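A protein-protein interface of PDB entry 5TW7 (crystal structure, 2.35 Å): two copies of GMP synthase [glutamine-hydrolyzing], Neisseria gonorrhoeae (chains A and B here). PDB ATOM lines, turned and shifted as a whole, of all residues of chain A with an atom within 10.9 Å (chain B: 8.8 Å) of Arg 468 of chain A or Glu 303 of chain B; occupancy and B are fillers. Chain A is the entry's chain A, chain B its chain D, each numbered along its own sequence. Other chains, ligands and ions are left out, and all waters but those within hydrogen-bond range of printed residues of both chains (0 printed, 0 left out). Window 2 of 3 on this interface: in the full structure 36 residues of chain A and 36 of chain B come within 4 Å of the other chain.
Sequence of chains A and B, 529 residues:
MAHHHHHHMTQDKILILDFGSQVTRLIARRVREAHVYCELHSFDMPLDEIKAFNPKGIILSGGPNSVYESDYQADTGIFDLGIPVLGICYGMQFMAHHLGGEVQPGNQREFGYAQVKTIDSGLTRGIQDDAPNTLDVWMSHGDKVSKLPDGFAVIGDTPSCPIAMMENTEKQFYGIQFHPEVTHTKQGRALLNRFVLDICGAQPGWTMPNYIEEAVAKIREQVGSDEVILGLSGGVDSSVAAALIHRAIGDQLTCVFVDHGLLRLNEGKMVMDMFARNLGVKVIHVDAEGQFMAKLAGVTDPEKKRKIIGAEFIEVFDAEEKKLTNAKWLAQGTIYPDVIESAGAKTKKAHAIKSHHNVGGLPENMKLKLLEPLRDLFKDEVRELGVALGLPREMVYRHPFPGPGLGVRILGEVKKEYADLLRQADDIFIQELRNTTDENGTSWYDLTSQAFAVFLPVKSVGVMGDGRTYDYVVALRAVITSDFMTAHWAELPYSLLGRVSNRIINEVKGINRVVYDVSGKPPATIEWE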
ATOM      1  N   LYS A 459      -1.085 -25.197 -12.433  1.00  0.00           N
ATOM      2  CA  LYS A 459      -0.844 -25.346 -13.857  1.00  0.00           C
ATOM      3  C   LYS A 459      -1.264 -24.099 -14.624  1.00  0.00           C
ATOM      4  O   LYS A 459      -2.247 -23.439 -14.277  1.00  0.00           O
ATOM      5  CB  LYS A 459      -1.548 -26.590 -14.400  1.00  0.00           C
ATOM      6  CG  LYS A 459      -0.970 -27.887 -13.812  1.00  0.00           C
ATOM      7  CD  LYS A 459      -0.877 -28.999 -14.843  1.00  0.00           C
ATOM      8  CE  LYS A 459      -0.687 -30.352 -14.172  1.00  0.00           C
ATOM      9  NZ  LYS A 459      -0.540 -31.479 -15.147  1.00  0.00           N
ATOM     10  N   SER A 460      -0.485 -23.773 -15.652  1.00  0.00           N
ATOM     11  CA  SER A 460      -0.741 -22.652 -16.539  1.00  0.00           C
ATOM     12  C   SER A 460      -0.808 -23.125 -17.985  1.00  0.00           C
ATOM     13  O   SER A 460      -0.181 -24.117 -18.360  1.00  0.00           O
ATOM     14  CB  SER A 460       0.364 -21.599 -16.370  1.00  0.00           C
ATOM     15  OG  SER A 460       0.406 -20.712 -17.455  1.00  0.00           O
ATOM     16  N   VAL A 461      -1.534 -22.388 -18.806  1.00  0.00           N
ATOM     17  CA  VAL A 461      -1.693 -22.732 -20.216  1.00  0.00           C
ATOM     18  C   VAL A 461      -0.522 -22.142 -20.998  1.00  0.00           C
ATOM     19  O   VAL A 461       0.122 -21.173 -20.571  1.00  0.00           O
ATOM     20  CB  VAL A 461      -3.044 -22.233 -20.755  1.00  0.00           C
ATOM     21  CG1 VAL A 461      -3.013 -20.735 -20.920  1.00  0.00           C
ATOM     22  CG2 VAL A 461      -3.384 -22.919 -22.066  1.00  0.00           C
ATOM     23  N   GLY A 462      -0.211 -22.760 -22.135  1.00  0.00           N
ATOM     24  CA  GLY A 462       0.874 -22.316 -22.989  1.00  0.00           C
ATOM     25  C   GLY A 462       0.672 -22.836 -24.394  1.00  0.00           C
ATOM     26  O   GLY A 462      -0.295 -23.544 -24.681  1.00  0.00           O
ATOM     27  N   VAL A 463       1.593 -22.464 -25.280  1.00  0.00           N
ATOM     28  CA  VAL A 463       1.523 -22.928 -26.666  1.00  0.00           C
ATOM     29  C   VAL A 463       2.673 -23.902 -26.949  1.00  0.00           C
ATOM     30  O   VAL A 463       3.791 -23.501 -27.285  1.00  0.00           O
ATOM     31  CB  VAL A 463       1.533 -21.751 -27.664  1.00  0.00           C
ATOM     32  N   GLY A 467      -1.060 -25.627 -31.195  1.00  0.00           N
ATOM     33  CA  GLY A 467      -0.746 -26.581 -30.141  1.00  0.00           C
ATOM     34  C   GLY A 467      -0.764 -26.004 -28.733  1.00  0.00           C
ATOM     35  O   GLY A 467       0.001 -25.089 -28.423  1.00  0.00           O
ATOM     36  N   ARG A 468      -1.620 -26.555 -27.872  1.00  0.00           N
ATOM     37  CA  ARG A 468      -1.861 -26.046 -26.525  1.00  0.00           C
ATOM     38  C   ARG A 468      -1.218 -26.953 -25.479  1.00  0.00           C
ATOM     39  O   ARG A 468      -1.275 -28.180 -25.596  1.00  0.00           O
ATOM     40  CB  ARG A 468      -3.373 -25.936 -26.273  1.00  0.00           C
ATOM     41  CG  ARG A 468      -3.786 -25.399 -24.904  1.00  0.00           C
ATOM     42  CD  ARG A 468      -5.305 -25.438 -24.743  1.00  0.00           C
ATOM     43  NE  ARG A 468      -5.785 -24.942 -23.450  1.00  0.00           N
ATOM     44  CZ  ARG A 468      -5.718 -25.622 -22.305  1.00  0.00           C
ATOM     45  NH1 ARG A 468      -6.196 -25.094 -21.186  1.00  0.00           N
ATOM     46  NH2 ARG A 468      -5.159 -26.824 -22.269  1.00  0.00           N
ATOM     47  N   THR A 469      -0.611 -26.352 -24.450  1.00  0.00           N
ATOM     48  CA  THR A 469       0.031 -27.093 -23.362  1.00  0.00           C
ATOM     49  C   THR A 469      -0.532 -26.645 -22.015  1.00  0.00           C
ATOM     50  O   THR A 469      -1.144 -25.579 -21.896  1.00  0.00           O
ATOM     51  CB  THR A 469       1.568 -26.916 -23.362  1.00  0.00           C
ATOM     52  OG1 THR A 469       1.913 -25.537 -23.149  1.00  0.00           O
ATOM     53  CG2 THR A 469       2.185 -27.411 -24.682  1.00  0.00           C
ATOM     54  N   TYR A 470      -0.311 -27.471 -20.984  1.00  0.00           N
ATOM     55  CA  TYR A 470      -0.893 -27.204 -19.665  1.00  0.00           C
ATOM     56  C   TYR A 470       0.012 -27.830 -18.597  1.00  0.00           C
ATOM     57  O   TYR A 470      -0.116 -29.021 -18.292  1.00  0.00           O
ATOM     58  CB  TYR A 470      -2.323 -27.741 -19.603  1.00  0.00           C
ATOM     59  CG  TYR A 470      -3.104 -27.271 -18.400  1.00  0.00           C
ATOM     60  CD1 TYR A 470      -3.275 -25.909 -18.151  1.00  0.00           C
ATOM     61  CD2 TYR A 470      -3.683 -28.174 -17.517  1.00  0.00           C
ATOM     62  CE1 TYR A 470      -3.986 -25.462 -17.043  1.00  0.00           C
ATOM     63  CE2 TYR A 470      -4.402 -27.735 -16.404  1.00  0.00           C
ATOM     64  CZ  TYR A 470      -4.550 -26.380 -16.176  1.00  0.00           C
ATOM     65  OH  TYR A 470      -5.258 -25.941 -15.083  1.00  0.00           O
ATOM     66  N   ASP A 471       0.921 -27.025 -18.030  1.00  0.00           N
ATOM     67  CA  ASP A 471       1.997 -27.527 -17.171  1.00  0.00           C
ATOM     68  C   ASP A 471       2.167 -26.657 -15.935  1.00  0.00           C
ATOM     69  O   ASP A 471       1.483 -25.642 -15.755  1.00  0.00           O
ATOM     70  CB  ASP A 471       3.329 -27.612 -17.921  1.00  0.00           C
ATOM     71  CG  ASP A 471       3.484 -28.899 -18.681  1.00  0.00           C
ATOM     72  OD1 ASP A 471       3.241 -29.977 -18.092  1.00  0.00           O
ATOM     73  OD2 ASP A 471       3.843 -28.822 -19.867  1.00  0.00           O
ATOM     74  N   ASN A 512       5.860 -24.828 -17.875  1.00  0.00           N
ATOM     75  CA  ASN A 512       5.676 -23.892 -18.984  1.00  0.00           C
ATOM     76  C   ASN A 512       5.452 -22.449 -18.523  1.00  0.00           C
ATOM     77  O   ASN A 512       5.015 -21.614 -19.312  1.00  0.00           O
ATOM     78  CB  ASN A 512       4.557 -24.349 -19.933  1.00  0.00           C
ATOM     79  CG  ASN A 512       3.177 -24.075 -19.410  1.00  0.00           C
ATOM     80  OD1 ASN A 512       2.984 -23.765 -18.230  1.00  0.00           O
ATOM     81  ND2 ASN A 512       2.189 -24.176 -20.305  1.00  0.00           N
ATOM     82  N   ARG A 513       5.785 -22.122 -17.281  1.00  0.00           N
ATOM     83  CA  ARG A 513       5.633 -20.753 -16.819  1.00  0.00           C
ATOM     84  C   ARG A 513       6.639 -20.492 -15.704  1.00  0.00           C
ATOM     85  O   ARG A 513       6.817 -21.325 -14.804  1.00  0.00           O
ATOM     86  CB  ARG A 513       4.186 -20.515 -16.362  1.00  0.00           C
ATOM     87  CG  ARG A 513       3.924 -19.195 -15.661  1.00  0.00           C
ATOM     88  CD  ARG A 513       3.328 -18.157 -16.559  1.00  0.00           C
ATOM     89  NE  ARG A 513       2.317 -18.679 -17.471  1.00  0.00           N
ATOM     90  CZ  ARG A 513       1.739 -17.933 -18.413  1.00  0.00           C
ATOM     91  NH1 ARG A 513       2.082 -16.652 -18.540  1.00  0.00           N
ATOM     92  NH2 ARG A 513       0.835 -18.457 -19.237  1.00  0.00           N
ATOM     93  N   LEU B 296     -19.923 -21.977 -11.295  1.00  0.00           N
ATOM     94  CA  LEU B 296     -18.503 -22.284 -11.368  1.00  0.00           C
ATOM     95  C   LEU B 296     -18.004 -23.116 -10.194  1.00  0.00           C
ATOM     96  O   LEU B 296     -16.850 -23.562 -10.225  1.00  0.00           O
ATOM     97  CB  LEU B 296     -17.694 -20.985 -11.461  1.00  0.00           C
ATOM     98  CG  LEU B 296     -17.718 -20.385 -12.861  1.00  0.00           C
ATOM     99  CD1 LEU B 296     -17.116 -18.985 -12.904  1.00  0.00           C
ATOM    100  CD2 LEU B 296     -16.973 -21.329 -13.761  1.00  0.00           C
ATOM    101  N   VAL B 299     -15.353 -26.257 -10.223  1.00  0.00           N
ATOM    102  CA  VAL B 299     -14.843 -26.416 -11.578  1.00  0.00           C
ATOM    103  C   VAL B 299     -13.419 -25.883 -11.621  1.00  0.00           C
ATOM    104  O   VAL B 299     -13.195 -24.684 -11.409  1.00  0.00           O
ATOM    105  CB  VAL B 299     -15.729 -25.682 -12.596  1.00  0.00           C
ATOM    106  CG1 VAL B 299     -15.141 -25.802 -13.999  1.00  0.00           C
ATOM    107  CG2 VAL B 299     -17.161 -26.232 -12.561  1.00  0.00           C
ATOM    108  N   THR B 300     -12.458 -26.768 -11.927  1.00  0.00           N
ATOM    109  CA  THR B 300     -11.047 -26.395 -11.990  1.00  0.00           C
ATOM    110  C   THR B 300     -10.468 -26.418 -13.396  1.00  0.00           C
ATOM    111  O   THR B 300      -9.455 -25.755 -13.628  1.00  0.00           O
ATOM    112  CB  THR B 300     -10.179 -27.305 -11.096  1.00  0.00           C
ATOM    113  OG1 THR B 300     -10.325 -28.673 -11.500  1.00  0.00           O
ATOM    114  CG2 THR B 300     -10.550 -27.162  -9.615  1.00  0.00           C
ATOM    115  N   ASP B 301     -11.036 -27.199 -14.311  1.00  0.00           N
ATOM    116  CA  ASP B 301     -10.543 -27.254 -15.681  1.00  0.00           C
ATOM    117  C   ASP B 301     -10.722 -25.885 -16.331  1.00  0.00           C
ATOM    118  O   ASP B 301     -11.857 -25.398 -16.427  1.00  0.00           O
ATOM    119  CB  ASP B 301     -11.293 -28.335 -16.465  1.00  0.00           C
ATOM    120  CG  ASP B 301     -10.710 -28.594 -17.861  1.00  0.00           C
ATOM    121  OD1 ASP B 301     -10.151 -27.681 -18.502  1.00  0.00           O
ATOM    122  OD2 ASP B 301     -10.828 -29.747 -18.327  1.00  0.00           O
ATOM    123  N   PRO B 302      -9.646 -25.228 -16.777  1.00  0.00           N
ATOM    124  CA  PRO B 302      -9.803 -23.883 -17.346  1.00  0.00           C
ATOM    125  C   PRO B 302     -10.643 -23.866 -18.608  1.00  0.00           C
ATOM    126  O   PRO B 302     -11.317 -22.869 -18.877  1.00  0.00           O
ATOM    127  CB  PRO B 302      -8.355 -23.434 -17.613  1.00  0.00           C
ATOM    128  CG  PRO B 302      -7.548 -24.670 -17.629  1.00  0.00           C
ATOM    129  CD  PRO B 302      -8.233 -25.639 -16.704  1.00  0.00           C
ATOM    130  N   GLU B 303     -10.607 -24.930 -19.407  1.00  0.00           N
ATOM    131  CA  GLU B 303     -11.424 -24.934 -20.611  1.00  0.00           C
ATOM    132  C   GLU B 303     -12.902 -25.001 -20.260  1.00  0.00           C
ATOM    133  O   GLU B 303     -13.714 -24.286 -20.853  1.00  0.00           O
ATOM    134  CB  GLU B 303     -11.008 -26.078 -21.534  1.00  0.00           C
ATOM    135  CG  GLU B 303      -9.716 -25.751 -22.290  1.00  0.00           C
ATOM    136  CD  GLU B 303      -9.093 -26.955 -22.970  1.00  0.00           C
ATOM    137  OE1 GLU B 303      -8.743 -26.844 -24.168  1.00  0.00           O
ATOM    138  OE2 GLU B 303      -8.946 -28.005 -22.304  1.00  0.00           O
ATOM    139  N   LYS B 304     -13.266 -25.811 -19.264  1.00  0.00           N
ATOM    140  CA  LYS B 304     -14.658 -25.832 -18.829  1.00  0.00           C
ATOM    141  C   LYS B 304     -15.074 -24.495 -18.216  1.00  0.00           C
ATOM    142  O   LYS B 304     -16.214 -24.047 -18.411  1.00  0.00           O
ATOM    143  CB  LYS B 304     -14.888 -26.985 -17.852  1.00  0.00           C
ATOM    144  CG  LYS B 304     -14.911 -28.354 -18.528  1.00  0.00           C
ATOM    145  CD  LYS B 304     -15.539 -29.409 -17.629  1.00  0.00           C
ATOM    146  CE  LYS B 304     -15.541 -30.788 -18.290  1.00  0.00           C
ATOM    147  NZ  LYS B 304     -15.367 -31.878 -17.283  1.00  0.00           N
ATOM    148  N   LYS B 305     -14.175 -23.843 -17.467  1.00  0.00           N
ATOM    149  CA  LYS B 305     -14.486 -22.527 -16.907  1.00  0.00           C
ATOM    150  C   LYS B 305     -14.845 -21.525 -17.998  1.00  0.00           C
ATOM    151  O   LYS B 305     -15.827 -20.783 -17.872  1.00  0.00           O
ATOM    152  CB  LYS B 305     -13.321 -22.002 -16.067  1.00  0.00           C
ATOM    153  CG  LYS B 305     -13.333 -22.507 -14.627  1.00  0.00           C
ATOM    154  CD  LYS B 305     -12.454 -21.651 -13.743  1.00  0.00           C
ATOM    155  CE  LYS B 305     -11.058 -21.595 -14.296  1.00  0.00           C
ATOM    156  NZ  LYS B 305     -10.204 -20.751 -13.450  1.00  0.00           N
ATOM    157  N   ARG B 306     -14.064 -21.492 -19.082  1.00  0.00           N
ATOM    158  CA  ARG B 306     -14.376 -20.582 -20.181  1.00  0.00           C
ATOM    159  C   ARG B 306     -15.720 -20.931 -20.807  1.00  0.00           C
ATOM    160  O   ARG B 306     -16.512 -20.038 -21.124  1.00  0.00           O
ATOM    161  CB  ARG B 306     -13.272 -20.616 -21.238  1.00  0.00           C
ATOM    162  CG  ARG B 306     -12.046 -19.799 -20.888  1.00  0.00           C
ATOM    163  CD  ARG B 306     -10.955 -20.057 -21.908  1.00  0.00           C
ATOM    164  NE  ARG B 306      -9.726 -19.323 -21.632  1.00  0.00           N
ATOM    165  CZ  ARG B 306      -9.514 -18.067 -22.000  1.00  0.00           C
ATOM    166  NH1 ARG B 306     -10.470 -17.405 -22.639  1.00  0.00           N
ATOM    167  NH2 ARG B 306      -8.359 -17.464 -21.708  1.00  0.00           N
ATOM    168  N   LYS B 307     -16.002 -22.230 -20.966  1.00  0.00           N
ATOM    169  CA  LYS B 307     -17.267 -22.668 -21.548  1.00  0.00           C
ATOM    170  C   LYS B 307     -18.449 -22.283 -20.662  1.00  0.00           C
ATOM    171  O   LYS B 307     -19.476 -21.799 -21.155  1.00  0.00           O
ATOM    172  CB  LYS B 307     -17.231 -24.180 -21.790  1.00  0.00           C
ATOM    173  N   ILE B 308     -18.325 -22.489 -19.349  1.00  0.00           N
ATOM    174  CA  ILE B 308     -19.417 -22.144 -18.444  1.00  0.00           C
ATOM    175  C   ILE B 308     -19.684 -20.646 -18.483  1.00  0.00           C
ATOM    176  O   ILE B 308     -20.831 -20.202 -18.623  1.00  0.00           O
ATOM    177  CB  ILE B 308     -19.105 -22.618 -17.016  1.00  0.00           C
ATOM    178  CG1 ILE B 308     -19.164 -24.139 -16.925  1.00  0.00           C
ATOM    179  CG2 ILE B 308     -20.062 -21.983 -16.040  1.00  0.00           C
ATOM    180  CD1 ILE B 308     -18.654 -24.693 -15.587  1.00  0.00           C
ATOM    181  N   ILE B 309     -18.623 -19.840 -18.385  1.00  0.00           N
ATOM    182  CA  ILE B 309     -18.811 -18.395 -18.293  1.00  0.00           C
ATOM    183  C   ILE B 309     -19.406 -17.844 -19.582  1.00  0.00           C
ATOM    184  O   ILE B 309     -20.327 -17.020 -19.546  1.00  0.00           O
ATOM    185  CB  ILE B 309     -17.496 -17.700 -17.907  1.00  0.00           C
ATOM    186  CG1 ILE B 309     -17.122 -18.101 -16.473  1.00  0.00           C
ATOM    187  CG2 ILE B 309     -17.626 -16.186 -18.045  1.00  0.00           C
ATOM    188  CD1 ILE B 309     -15.684 -17.816 -16.115  1.00  0.00           C
ATOM    189  N   GLY B 310     -18.913 -18.297 -20.737  1.00  0.00           N
ATOM    190  CA  GLY B 310     -19.443 -17.797 -21.997  1.00  0.00           C
ATOM    191  C   GLY B 310     -20.902 -18.171 -22.219  1.00  0.00           C
ATOM    192  O   GLY B 310     -21.721 -17.330 -22.592  1.00  0.00           O
ATOM    193  N   PRO B 404     -14.147 -13.937 -20.326  1.00  0.00           N
ATOM    194  CA  PRO B 404     -14.322 -14.630 -19.037  1.00  0.00           C
ATOM    195  C   PRO B 404     -13.748 -13.887 -17.838  1.00  0.00           C
ATOM    196  O   PRO B 404     -13.787 -14.435 -16.731  1.00  0.00           O
ATOM    197  CB  PRO B 404     -13.606 -15.972 -19.263  1.00  0.00           C
ATOM    198  CG  PRO B 404     -12.651 -15.706 -20.376  1.00  0.00           C
ATOM    199  CD  PRO B 404     -13.320 -14.717 -21.265  1.00  0.00           C
ATOM    200  N   GLY B 407     -12.290 -14.832 -14.221  1.00  0.00           N
ATOM    201  CA  GLY B 407     -12.428 -16.278 -14.265  1.00  0.00           C
ATOM    202  C   GLY B 407     -11.220 -17.007 -14.827  1.00  0.00           C
ATOM    203  O   GLY B 407     -11.008 -18.184 -14.519  1.00  0.00           O
ATOM    204  N   VAL B 408     -10.445 -16.348 -15.692  1.00  0.00           N
ATOM    205  CA  VAL B 408      -9.194 -16.910 -16.197  1.00  0.00           C
ATOM    206  C   VAL B 408      -7.982 -16.302 -15.505  1.00  0.00           C
ATOM    207  O   VAL B 408      -6.851 -16.509 -15.956  1.00  0.00           O
ATOM    208  CB  VAL B 408      -9.063 -16.737 -17.716  1.00  0.00           C
ATOM    209  CG1 VAL B 408     -10.126 -17.509 -18.432  1.00  0.00           C
ATOM    210  CG2 VAL B 408      -9.107 -15.255 -18.075  1.00  0.00           C
ATOM    211  N   PRO B 523       7.388 -18.442 -25.355  1.00  0.00           N
ATOM    212  CA  PRO B 523       6.637 -19.710 -25.380  1.00  0.00           C
ATOM    213  C   PRO B 523       5.373 -19.763 -24.528  1.00  0.00           C
ATOM    214  O   PRO B 523       4.662 -20.763 -24.568  1.00  0.00           O
ATOM    215  CB  PRO B 523       7.662 -20.708 -24.842  1.00  0.00           C
ATOM    216  CG  PRO B 523       8.451 -19.895 -23.841  1.00  0.00           C
ATOM    217  CD  PRO B 523       8.433 -18.451 -24.316  1.00  0.00           C
ATOM    218  N   THR B 525       1.613 -17.914 -23.001  1.00  0.00           N
ATOM    219  CA  THR B 525       0.509 -17.040 -23.361  1.00  0.00           C
ATOM    220  C   THR B 525       0.442 -15.869 -22.383  1.00  0.00           C
ATOM    221  O   THR B 525       1.063 -15.887 -21.313  1.00  0.00           O
ATOM    222  CB  THR B 525      -0.812 -17.802 -23.337  1.00  0.00           C
ATOM    223  OG1 THR B 525      -0.947 -18.392 -22.041  1.00  0.00           O
ATOM    224  CG2 THR B 525      -0.865 -18.882 -24.431  1.00  0.00           C
ATOM    225  N   TRP B 528      -2.952 -16.705 -18.005  1.00  0.00           N
ATOM    226  CA  TRP B 528      -2.495 -17.980 -17.467  1.00  0.00           C
ATOM    227  C   TRP B 528      -3.456 -19.124 -17.753  1.00  0.00           C
ATOM    228  O   TRP B 528      -3.036 -20.285 -17.731  1.00  0.00           O
ATOM    229  CB  TRP B 528      -2.285 -17.880 -15.961  1.00  0.00           C
ATOM    230  CG  TRP B 528      -1.034 -17.154 -15.554  1.00  0.00           C
ATOM    231  CD1 TRP B 528      -0.515 -16.031 -16.122  1.00  0.00           C
ATOM    232  CD2 TRP B 528      -0.175 -17.483 -14.460  1.00  0.00           C
ATOM    233  NE1 TRP B 528       0.625 -15.644 -15.460  1.00  0.00           N
ATOM    234  CE2 TRP B 528       0.859 -16.524 -14.436  1.00  0.00           C
ATOM    235  CE3 TRP B 528      -0.170 -18.502 -13.503  1.00  0.00           C
ATOM    236  CZ2 TRP B 528       1.885 -16.556 -13.493  1.00  0.00           C
ATOM    237  CZ3 TRP B 528       0.859 -18.532 -12.557  1.00  0.00           C
ATOM    238  CH2 TRP B 528       1.866 -17.565 -12.560  1.00  0.00           C
ATOM    239  N   GLU B 529      -4.713 -18.831 -18.061  1.00  0.00           N
ATOM    240  CA  GLU B 529      -5.693 -19.886 -18.335  1.00  0.00           C
ATOM    241  C   GLU B 529      -6.517 -19.555 -19.585  1.00  0.00           C
ATOM    242  O   GLU B 529      -6.395 -18.441 -20.115  1.00  0.00           O
ATOM    243  CB  GLU B 529      -6.624 -20.087 -17.142  1.00  0.00           C
ATOM    244  CG  GLU B 529      -6.073 -21.000 -16.052  1.00  0.00           C
ATOM    245  CD  GLU B 529      -7.078 -21.224 -14.932  1.00  0.00           C
ATOM    246  OE1 GLU B 529      -7.990 -20.377 -14.786  1.00  0.00           O
ATOM    247  OE2 GLU B 529      -6.975 -22.248 -14.220  1.00  0.00           O
ATOM    248  OXT GLU B 529      -7.309 -20.379 -20.078  1.00  0.00           O
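The guanidinium group (NE) of Arg 468 of chain A lies within salt-bridge range of the side-chain carboxylate (OE1) of Glu 303 of chain B. The backbone carbonyl oxygen (O) of Val 461 of chain A lies close to the side-chain hydroxyl (OG1) of Thr 525 of chain B. The backbone carbonyl oxygen (O) of Trp 528 of chain B lies within hydrogen-bond range of the backbone NH (N) of Val 461 of chain A (2.8 Å). The backbone carbonyl oxygen of Thr 525 of chain B sits at hydrogen-bond distance from the guanidinium group of Arg 513 of chain A (3.1 Å). The backbone carbonyl oxygen (O) of Trp 528 of chain B sits at hydrogen-bond distance from the side-chain hydroxyl (OG) of Ser 460 of chain A (3.5 Å).
The side-chain hydroxyl (OG) of Ser 460 of chain A is in hydrogen-bond range of the guanidinium group (NE) of Arg 513 of chain A, at 2.8 Å. The backbone carbonyl oxygen (O) of Ser 460 of chain A lies within hydrogen-bond range of the side-chain amide nitrogen (ND2) of Asn 512 of chain A (3.1 Å). O of Asp 471 of chain A lies within hydrogen-bond range of N of Ser 460 of chain A. The side-chain carboxylate (OD1) of Asp 301 of chain B lies within hydrogen-bond range of the backbone NH (N) of Glu 303 of chain B, at 2.9 Å. The guanidinium group of Arg 306 of chain B lies within salt-bridge range of the chain-end carboxylate of Glu 529 of chain B, at 2.7 Å. NZ of Lys 305 of chain B lies within salt-bridge range of OE1 of Glu 529 of chain B (2.6 Å).
Val 461 of chain A touches Glu 529 of chain B (CG1 to CA, 3.8 Å). Val 463 of chain A touches Pro 523 of chain B (N to O, 3.6 Å). Pro 302 of chain B touches Arg 468 of chain A. Pro 302 of chain B touches Tyr 470 of chain A (CD to OH, 3.4 Å). Trp 528 of chain B touches Arg 513 of chain A.
Printed residues of chain B within 4 Å of Val 461 of chain A: Thr 525 (3.3 Å), Trp 528 (2.8 Å) and Glu 529 (3.8 Å). Of the printed residues of chain B, Val 463 of chain A touches Pro 523. Arg 468 of chain A touches two residues of chain B. No residue of chain B comes within 4 Å of Thr 469 of chain A. No residue of chain A comes within 4 Å of Asp 301 of chain B. Pro 302 of chain B touches just these residues of chain A: Arg 468 and Tyr 470. No residue of chain A comes within 4 Å of Lys 307 of chain B. The nearest printed residue of chain B that does not touch Tyr 470 of chain A is Glu 529 of chain B (4.2 Å).
Hydrophobic or aromatic side chains of chain B within 4 Å of the printed part of chain A: Pro 302 and Trp 528. Along chain B the printed residues that touch a printed residue of chain A span positions 302 to 529. Of the 12 printed residues of chain A, 6 touch a printed residue of chain B.
No position is printed for both chains. Of the 10 pairs that touch across the chains among the printed residues, none has its exchanged pair printed and touching as well.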
